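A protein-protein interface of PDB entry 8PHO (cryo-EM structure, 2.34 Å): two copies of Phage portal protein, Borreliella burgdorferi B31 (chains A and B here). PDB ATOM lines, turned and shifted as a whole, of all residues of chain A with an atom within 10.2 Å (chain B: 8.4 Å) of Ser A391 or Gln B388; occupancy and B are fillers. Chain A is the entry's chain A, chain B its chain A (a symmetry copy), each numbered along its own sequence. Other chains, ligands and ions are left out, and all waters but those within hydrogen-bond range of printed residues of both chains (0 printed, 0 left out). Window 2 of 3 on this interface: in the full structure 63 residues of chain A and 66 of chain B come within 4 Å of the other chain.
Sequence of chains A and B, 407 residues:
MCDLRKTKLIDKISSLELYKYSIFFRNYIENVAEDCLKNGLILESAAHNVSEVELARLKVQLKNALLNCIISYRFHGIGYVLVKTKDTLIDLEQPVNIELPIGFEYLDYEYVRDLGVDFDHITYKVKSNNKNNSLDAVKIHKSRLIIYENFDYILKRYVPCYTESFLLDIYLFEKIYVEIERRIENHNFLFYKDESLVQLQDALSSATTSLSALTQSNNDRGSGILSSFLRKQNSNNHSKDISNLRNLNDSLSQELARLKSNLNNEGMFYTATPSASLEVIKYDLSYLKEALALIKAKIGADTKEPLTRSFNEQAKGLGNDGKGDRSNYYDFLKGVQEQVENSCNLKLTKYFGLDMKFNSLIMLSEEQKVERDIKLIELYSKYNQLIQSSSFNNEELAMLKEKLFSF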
ATOM      1  N   GLN A 385      12.613 -16.441  33.401  1.00  0.00           N
ATOM      2  CA  GLN A 385      11.635 -16.851  32.399  1.00  0.00           C
ATOM      3  C   GLN A 385      12.230 -17.869  31.432  1.00  0.00           C
ATOM      4  O   GLN A 385      11.561 -18.832  31.043  1.00  0.00           O
ATOM      5  CB  GLN A 385      11.119 -15.631  31.642  1.00  0.00           C
ATOM      6  CG  GLN A 385       9.992 -15.945  30.680  1.00  0.00           C
ATOM      7  CD  GLN A 385       9.396 -14.698  30.059  1.00  0.00           C
ATOM      8  OE1 GLN A 385       9.768 -13.580  30.413  1.00  0.00           O
ATOM      9  NE2 GLN A 385       8.399 -14.882  29.204  1.00  0.00           N
ATOM     10  N   LEU A 386      13.488 -17.671  31.032  1.00  0.00           N
ATOM     11  CA  LEU A 386      14.157 -18.637  30.167  1.00  0.00           C
ATOM     12  C   LEU A 386      14.284 -19.997  30.842  1.00  0.00           C
ATOM     13  O   LEU A 386      14.013 -21.035  30.226  1.00  0.00           O
ATOM     14  CB  LEU A 386      15.537 -18.113  29.772  1.00  0.00           C
ATOM     15  CG  LEU A 386      16.374 -19.090  28.942  1.00  0.00           C
ATOM     16  CD1 LEU A 386      15.684 -19.531  27.666  1.00  0.00           C
ATOM     17  CD2 LEU A 386      17.745 -18.489  28.650  1.00  0.00           C
ATOM     18  N   ILE A 387      14.693 -20.011  32.106  1.00  0.00           N
ATOM     19  CA  ILE A 387      14.918 -21.268  32.808  1.00  0.00           C
ATOM     20  C   ILE A 387      13.600 -22.006  33.007  1.00  0.00           C
ATOM     21  O   ILE A 387      13.514 -23.222  32.792  1.00  0.00           O
ATOM     22  CB  ILE A 387      15.645 -21.023  34.141  1.00  0.00           C
ATOM     23  CG1 ILE A 387      17.062 -20.498  33.904  1.00  0.00           C
ATOM     24  CG2 ILE A 387      15.724 -22.317  34.943  1.00  0.00           C
ATOM     25  CD1 ILE A 387      17.973 -21.447  33.177  1.00  0.00           C
ATOM     26  N   GLN A 388      12.537 -21.270  33.333  1.00  0.00           N
ATOM     27  CA  GLN A 388      11.277 -21.905  33.693  1.00  0.00           C
ATOM     28  C   GLN A 388      10.589 -22.495  32.468  1.00  0.00           C
ATOM     29  O   GLN A 388       9.992 -23.575  32.547  1.00  0.00           O
ATOM     30  CB  GLN A 388      10.349 -20.914  34.393  1.00  0.00           C
ATOM     31  CG  GLN A 388      10.716 -20.593  35.834  1.00  0.00           C
ATOM     32  CD  GLN A 388       9.645 -19.755  36.506  1.00  0.00           C
ATOM     33  OE1 GLN A 388       9.887 -19.101  37.521  1.00  0.00           O
ATOM     34  NE2 GLN A 388       8.451 -19.746  35.919  1.00  0.00           N
ATOM     35  N   SER A 389      10.669 -21.814  31.325  1.00  0.00           N
ATOM     36  CA  SER A 389       9.937 -22.219  30.129  1.00  0.00           C
ATOM     37  C   SER A 389      10.855 -22.808  29.064  1.00  0.00           C
ATOM     38  O   SER A 389      10.735 -22.476  27.884  1.00  0.00           O
ATOM     39  CB  SER A 389       9.155 -21.042  29.548  1.00  0.00           C
ATOM     40  OG  SER A 389      10.045 -20.016  29.138  1.00  0.00           O
ATOM     41  N   SER A 390      11.810 -23.654  29.448  1.00  0.00           N
ATOM     42  CA  SER A 390      12.669 -24.272  28.447  1.00  0.00           C
ATOM     43  C   SER A 390      12.888 -25.725  28.835  1.00  0.00           C
ATOM     44  O   SER A 390      12.535 -26.155  29.935  1.00  0.00           O
ATOM     45  CB  SER A 390      14.017 -23.554  28.306  1.00  0.00           C
ATOM     46  OG  SER A 390      14.862 -23.832  29.412  1.00  0.00           O
ATOM     47  N   SER A 391      13.504 -26.480  27.931  1.00  0.00           N
ATOM     48  CA  SER A 391      13.819 -27.883  28.175  1.00  0.00           C
ATOM     49  C   SER A 391      15.256 -28.194  27.778  1.00  0.00           C
ATOM     50  O   SER A 391      15.538 -29.218  27.154  1.00  0.00           O
ATOM     51  CB  SER A 391      12.848 -28.799  27.434  1.00  0.00           C
ATOM     52  OG  SER A 391      12.876 -28.523  26.043  1.00  0.00           O
ATOM     53  N   PHE A 392      16.180 -27.290  28.090  1.00  0.00           N
ATOM     54  CA  PHE A 392      17.583 -27.462  27.743  1.00  0.00           C
ATOM     55  C   PHE A 392      18.237 -28.533  28.622  1.00  0.00           C
ATOM     56  O   PHE A 392      17.996 -28.598  29.828  1.00  0.00           O
ATOM     57  CB  PHE A 392      18.299 -26.116  27.897  1.00  0.00           C
ATOM     58  CG  PHE A 392      18.096 -25.172  26.729  1.00  0.00           C
ATOM     59  CD1 PHE A 392      18.566 -25.456  25.453  1.00  0.00           C
ATOM     60  CD2 PHE A 392      17.427 -23.974  26.936  1.00  0.00           C
ATOM     61  CE1 PHE A 392      18.356 -24.544  24.418  1.00  0.00           C
ATOM     62  CE2 PHE A 392      17.224 -23.070  25.919  1.00  0.00           C
ATOM     63  CZ  PHE A 392      17.638 -23.371  24.655  1.00  0.00           C
ATOM     64  N   ASN A 393      19.076 -29.382  28.020  1.00  0.00           N
ATOM     65  CA  ASN A 393      19.815 -30.337  28.832  1.00  0.00           C
ATOM     66  C   ASN A 393      20.678 -29.609  29.866  1.00  0.00           C
ATOM     67  O   ASN A 393      21.139 -28.487  29.641  1.00  0.00           O
ATOM     68  CB  ASN A 393      20.697 -31.213  27.936  1.00  0.00           C
ATOM     69  CG  ASN A 393      19.887 -32.178  27.057  1.00  0.00           C
ATOM     70  OD1 ASN A 393      18.773 -32.566  27.393  1.00  0.00           O
ATOM     71  ND2 ASN A 393      20.516 -32.649  25.972  1.00  0.00           N
ATOM     72  N   ASN A 394      20.912 -30.258  31.012  1.00  0.00           N
ATOM     73  CA  ASN A 394      21.621 -29.574  32.093  1.00  0.00           C
ATOM     74  C   ASN A 394      22.973 -29.028  31.618  1.00  0.00           C
ATOM     75  O   ASN A 394      23.324 -27.877  31.912  1.00  0.00           O
ATOM     76  CB  ASN A 394      21.794 -30.501  33.298  1.00  0.00           C
ATOM     77  CG  ASN A 394      22.306 -29.750  34.563  1.00  0.00           C
ATOM     78  OD1 ASN A 394      22.475 -28.524  34.545  1.00  0.00           O
ATOM     79  ND2 ASN A 394      22.646 -30.499  35.609  1.00  0.00           N
ATOM     80  N   GLU A 395      23.732 -29.837  30.879  1.00  0.00           N
ATOM     81  CA  GLU A 395      25.041 -29.404  30.399  1.00  0.00           C
ATOM     82  C   GLU A 395      24.942 -28.083  29.640  1.00  0.00           C
ATOM     83  O   GLU A 395      25.672 -27.126  29.936  1.00  0.00           O
ATOM     84  CB  GLU A 395      25.643 -30.494  29.515  1.00  0.00           C
ATOM     85  CG  GLU A 395      25.757 -31.858  30.167  1.00  0.00           C
ATOM     86  CD  GLU A 395      26.548 -32.868  29.336  1.00  0.00           C
ATOM     87  OE1 GLU A 395      26.922 -32.556  28.182  1.00  0.00           O
ATOM     88  OE2 GLU A 395      26.722 -34.005  29.818  1.00  0.00           O
ATOM     89  N   GLU A 396      24.002 -28.001  28.696  1.00  0.00           N
ATOM     90  CA  GLU A 396      23.782 -26.761  27.959  1.00  0.00           C
ATOM     91  C   GLU A 396      23.490 -25.599  28.897  1.00  0.00           C
ATOM     92  O   GLU A 396      24.033 -24.500  28.729  1.00  0.00           O
ATOM     93  CB  GLU A 396      22.635 -26.949  26.980  1.00  0.00           C
ATOM     94  CG  GLU A 396      22.632 -28.275  26.249  1.00  0.00           C
ATOM     95  CD  GLU A 396      21.473 -28.407  25.290  1.00  0.00           C
ATOM     96  OE1 GLU A 396      20.358 -28.712  25.761  1.00  0.00           O
ATOM     97  OE2 GLU A 396      21.675 -28.219  24.072  1.00  0.00           O
ATOM     98  N   LEU A 397      22.670 -25.850  29.918  1.00  0.00           N
ATOM     99  CA  LEU A 397      22.396 -24.837  30.929  1.00  0.00           C
ATOM    100  C   LEU A 397      23.666 -24.426  31.665  1.00  0.00           C
ATOM    101  O   LEU A 397      23.892 -23.234  31.904  1.00  0.00           O
ATOM    102  CB  LEU A 397      21.345 -25.348  31.913  1.00  0.00           C
ATOM    103  CG  LEU A 397      19.939 -25.524  31.332  1.00  0.00           C
ATOM    104  CD1 LEU A 397      19.010 -26.204  32.328  1.00  0.00           C
ATOM    105  CD2 LEU A 397      19.365 -24.210  30.851  1.00  0.00           C
ATOM    106  N   TYR B 380      18.889 -17.524  23.257  1.00  0.00           N
ATOM    107  CA  TYR B 380      18.600 -18.863  23.757  1.00  0.00           C
ATOM    108  C   TYR B 380      17.100 -19.117  23.803  1.00  0.00           C
ATOM    109  O   TYR B 380      16.642 -20.218  23.479  1.00  0.00           O
ATOM    110  CB  TYR B 380      19.221 -19.053  25.138  1.00  0.00           C
ATOM    111  CG  TYR B 380      20.558 -19.753  25.107  1.00  0.00           C
ATOM    112  CD1 TYR B 380      21.615 -19.239  24.372  1.00  0.00           C
ATOM    113  CD2 TYR B 380      20.769 -20.922  25.831  1.00  0.00           C
ATOM    114  CE1 TYR B 380      22.830 -19.892  24.329  1.00  0.00           C
ATOM    115  CE2 TYR B 380      21.986 -21.583  25.790  1.00  0.00           C
ATOM    116  CZ  TYR B 380      23.027 -21.025  25.088  1.00  0.00           C
ATOM    117  OH  TYR B 380      24.268 -21.615  25.021  1.00  0.00           O
ATOM    118  N   SER B 381      16.317 -18.113  24.204  1.00  0.00           N
ATOM    119  CA  SER B 381      14.863 -18.251  24.189  1.00  0.00           C
ATOM    120  C   SER B 381      14.330 -18.464  22.782  1.00  0.00           C
ATOM    121  O   SER B 381      13.437 -19.291  22.568  1.00  0.00           O
ATOM    122  CB  SER B 381      14.220 -17.018  24.811  1.00  0.00           C
ATOM    123  OG  SER B 381      12.805 -17.107  24.762  1.00  0.00           O
ATOM    124  N   LYS B 382      14.844 -17.714  21.809  1.00  0.00           N
ATOM    125  CA  LYS B 382      14.397 -17.910  20.436  1.00  0.00           C
ATOM    126  C   LYS B 382      14.759 -19.303  19.930  1.00  0.00           C
ATOM    127  O   LYS B 382      13.952 -19.950  19.251  1.00  0.00           O
ATOM    128  CB  LYS B 382      14.996 -16.829  19.546  1.00  0.00           C
ATOM    129  CG  LYS B 382      14.416 -15.442  19.777  1.00  0.00           C
ATOM    130  CD  LYS B 382      12.930 -15.389  19.524  1.00  0.00           C
ATOM    131  CE  LYS B 382      12.402 -13.973  19.715  1.00  0.00           C
ATOM    132  NZ  LYS B 382      11.046 -13.800  19.125  1.00  0.00           N
ATOM    133  N   TYR B 383      15.954 -19.783  20.277  1.00  0.00           N
ATOM    134  CA  TYR B 383      16.363 -21.121  19.870  1.00  0.00           C
ATOM    135  C   TYR B 383      15.469 -22.188  20.489  1.00  0.00           C
ATOM    136  O   TYR B 383      15.085 -23.150  19.816  1.00  0.00           O
ATOM    137  CB  TYR B 383      17.825 -21.361  20.245  1.00  0.00           C
ATOM    138  CG  TYR B 383      18.369 -22.672  19.731  1.00  0.00           C
ATOM    139  CD1 TYR B 383      18.371 -22.965  18.376  1.00  0.00           C
ATOM    140  CD2 TYR B 383      18.908 -23.608  20.605  1.00  0.00           C
ATOM    141  CE1 TYR B 383      18.863 -24.167  17.909  1.00  0.00           C
ATOM    142  CE2 TYR B 383      19.395 -24.815  20.147  1.00  0.00           C
ATOM    143  CZ  TYR B 383      19.415 -25.067  18.795  1.00  0.00           C
ATOM    144  OH  TYR B 383      19.896 -26.273  18.342  1.00  0.00           O
ATOM    145  N   ASN B 384      15.119 -22.024  21.767  1.00  0.00           N
ATOM    146  CA  ASN B 384      14.237 -22.984  22.420  1.00  0.00           C
ATOM    147  C   ASN B 384      12.849 -22.974  21.796  1.00  0.00           C
ATOM    148  O   ASN B 384      12.252 -24.034  21.581  1.00  0.00           O
ATOM    149  CB  ASN B 384      14.159 -22.686  23.914  1.00  0.00           C
ATOM    150  CG  ASN B 384      13.142 -23.552  24.626  1.00  0.00           C
ATOM    151  OD1 ASN B 384      13.410 -24.709  24.942  1.00  0.00           O
ATOM    152  ND2 ASN B 384      11.966 -22.990  24.888  1.00  0.00           N
ATOM    153  N   GLN B 385      12.334 -21.788  21.463  1.00  0.00           N
ATOM    154  CA  GLN B 385      11.032 -21.709  20.812  1.00  0.00           C
ATOM    155  C   GLN B 385      11.064 -22.358  19.432  1.00  0.00           C
ATOM    156  O   GLN B 385      10.114 -23.043  19.037  1.00  0.00           O
ATOM    157  CB  GLN B 385      10.587 -20.252  20.708  1.00  0.00           C
ATOM    158  CG  GLN B 385       9.180 -20.083  20.176  1.00  0.00           C
ATOM    159  CD  GLN B 385       8.709 -18.644  20.228  1.00  0.00           C
ATOM    160  OE1 GLN B 385       9.407 -17.774  20.748  1.00  0.00           O
ATOM    161  NE2 GLN B 385       7.483 -18.405  19.783  1.00  0.00           N
ATOM    162  N   LEU B 386      12.149 -22.152  18.683  1.00  0.00           N
ATOM    163  CA  LEU B 386      12.292 -22.798  17.382  1.00  0.00           C
ATOM    164  C   LEU B 386      12.319 -24.315  17.512  1.00  0.00           C
ATOM    165  O   LEU B 386      11.653 -25.026  16.751  1.00  0.00           O
ATOM    166  CB  LEU B 386      13.564 -22.304  16.694  1.00  0.00           C
ATOM    167  CG  LEU B 386      13.871 -22.989  15.359  1.00  0.00           C
ATOM    168  CD1 LEU B 386      12.744 -22.865  14.352  1.00  0.00           C
ATOM    169  CD2 LEU B 386      15.183 -22.459  14.789  1.00  0.00           C
ATOM    170  N   ILE B 387      13.084 -24.828  18.471  1.00  0.00           N
ATOM    171  CA  ILE B 387      13.233 -26.270  18.620  1.00  0.00           C
ATOM    172  C   ILE B 387      11.913 -26.898  19.048  1.00  0.00           C
ATOM    173  O   ILE B 387      11.502 -27.937  18.517  1.00  0.00           O
ATOM    174  CB  ILE B 387      14.369 -26.599  19.604  1.00  0.00           C
ATOM    175  CG1 ILE B 387      15.724 -26.165  19.041  1.00  0.00           C
ATOM    176  CG2 ILE B 387      14.406 -28.098  19.883  1.00  0.00           C
ATOM    177  CD1 ILE B 387      16.137 -26.869  17.779  1.00  0.00           C
ATOM    178  N   GLN B 388      11.189 -26.231  19.948  1.00  0.00           N
ATOM    179  CA  GLN B 388       9.994 -26.826  20.528  1.00  0.00           C
ATOM    180  C   GLN B 388       8.851 -26.859  19.520  1.00  0.00           C
ATOM    181  O   GLN B 388       8.086 -27.830  19.475  1.00  0.00           O
ATOM    182  CB  GLN B 388       9.565 -26.072  21.786  1.00  0.00           C
ATOM    183  CG  GLN B 388      10.417 -26.334  23.018  1.00  0.00           C
ATOM    184  CD  GLN B 388       9.815 -25.698  24.256  1.00  0.00           C
ATOM    185  OE1 GLN B 388      10.493 -25.486  25.261  1.00  0.00           O
ATOM    186  NE2 GLN B 388       8.530 -25.359  24.177  1.00  0.00           N
ATOM    187  N   SER B 389       8.723 -25.821  18.694  1.00  0.00           N
ATOM    188  CA  SER B 389       7.589 -25.690  17.785  1.00  0.00           C
ATOM    189  C   SER B 389       7.984 -25.936  16.334  1.00  0.00           C
ATOM    190  O   SER B 389       7.583 -25.189  15.441  1.00  0.00           O
ATOM    191  CB  SER B 389       6.943 -24.311  17.919  1.00  0.00           C
ATOM    192  OG  SER B 389       7.866 -23.298  17.550  1.00  0.00           O
ATOM    193  N   SER B 390       8.801 -26.954  16.064  1.00  0.00           N
ATOM    194  CA  SER B 390       9.155 -27.246  14.681  1.00  0.00           C
ATOM    195  C   SER B 390       9.160 -28.755  14.496  1.00  0.00           C
ATOM    196  O   SER B 390       9.077 -29.519  15.460  1.00  0.00           O
ATOM    197  CB  SER B 390      10.517 -26.661  14.287  1.00  0.00           C
ATOM    198  OG  SER B 390      11.579 -27.405  14.867  1.00  0.00           O
ATOM    199  N   SER B 391       9.288 -29.186  13.246  1.00  0.00           N
ATOM    200  CA  SER B 391       9.348 -30.605  12.915  1.00  0.00           C
ATOM    201  C   SER B 391      10.490 -30.889  11.948  1.00  0.00           C
ATOM    202  O   SER B 391      10.335 -31.638  10.983  1.00  0.00           O
ATOM    203  CB  SER B 391       8.022 -31.089  12.336  1.00  0.00           C
ATOM    204  OG  SER B 391       7.680 -30.330  11.187  1.00  0.00           O
ATOM    205  N   LEU B 397      18.526 -30.221  11.852  1.00  0.00           N
ATOM    206  CA  LEU B 397      18.804 -29.624  13.151  1.00  0.00           C
ATOM    207  C   LEU B 397      20.296 -29.635  13.462  1.00  0.00           C
ATOM    208  O   LEU B 397      20.839 -28.640  13.957  1.00  0.00           O
ATOM    209  CB  LEU B 397      18.021 -30.353  14.242  1.00  0.00           C
ATOM    210  CG  LEU B 397      16.502 -30.167  14.188  1.00  0.00           C
ATOM    211  CD1 LEU B 397      15.799 -31.068  15.194  1.00  0.00           C
ATOM    212  CD2 LEU B 397      16.109 -28.719  14.378  1.00  0.00           C
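O of Ser A389 sits at hydrogen-bond distance from ND2 of Asn B384. OD1 of Asn B384 is in hydrogen-bond range of N of Ser A391 (3.5 Å).
The side-chain amide nitrogen (ND2) of Asn B384 is in hydrogen-bond range of the side-chain amide oxygen (OE1) of Gln B388 (2.9 Å). The side-chain hydroxyl (OG) of Ser A390 lies within hydrogen-bond range of the backbone carbonyl oxygen (O) of Leu A386 (3.0 Å). The backbone carbonyl oxygen (O) of Gln A385 lies within hydrogen-bond range of the side-chain hydroxyl (OG) of Ser A389 (2.7 Å).
Leu A386 touches Tyr B380. Ser B381 touches Leu A386. Ser A389 touches Gln B388 (O to OE1, 3.9998 Å). OD1 of Asn B384 touches CB of Ser A390, 3.6 Å away. Ser A391 touches Gln B388 (OG to OE1, 3.9 Å). Phe A392 touches Tyr B380 (CZ to O, 3.5 Å). Phe A392 touches Tyr B383. Phe A392 touches Asn B384.
Ser A391 touches two residues of chain B. Printed residues of chain A within 4 Å of Asn B384: Ser A389 (3.3 Å), Ser A390 (3.6 Å), Ser A391 (3.5 Å) and Phe A392 (3.6 Å). No residue of chain A comes within 4 Å of Ile B387. No residue of chain A comes within 4 Å of Ser B390. Of the printed residues of chain A, Tyr B380 touches Leu A386 and Phe A392. Of the printed residues of chain A, Ser B381 touches Leu A386. Of the printed residues of chain B, Leu A386 touches Tyr B380 (3.9 Å) and Ser B381 (3.8 Å). Of the printed residues of chain A, Tyr B383 touches Phe A392 (3.96 Å). The nearest printed residue of chain A that does not touch Gln B388 is Ser A390 (4.04 Å). The nearest printed residue of chain B that does not touch Ser A389 is Ser B381 (5.9 Å).
Of the 13 printed residues of chain B, 5 touch a printed residue of chain A. Printed residues of chain B that touch a printed residue of chain A: Tyr B380, Ser B381, Tyr B383, Asn B384 and Gln B388. Hydrophobic or aromatic side chains of chain B that line the printed part of chain A: Tyr B380 and Tyr B383. Of the 13 printed residues of chain A, 5 touch a printed residue of chain B. Hydrophobic or aromatic side chains of chain A that line the printed part of chain B: Leu A386 and Phe A392. Among the printed residues, no Asp or Glu carboxylate lies within 4 Å of a Lys or Arg side-chain nitrogen of the other chain.
Ser A389 touches Gln B388, but with the chains exchanged Gln A388 does not touch Ser B389 (14.1 Å). Ser A391 touches Gln B388, but with the chains exchanged Gln A388 does not touch Ser B391 (20.1 Å). Positions printed for both chains: 385, 386, 387, 388, 389, 390, 391 and 397. Of the 10 pairs that touch across the chains among the printed residues, none has its exchanged pair printed and touching as well.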
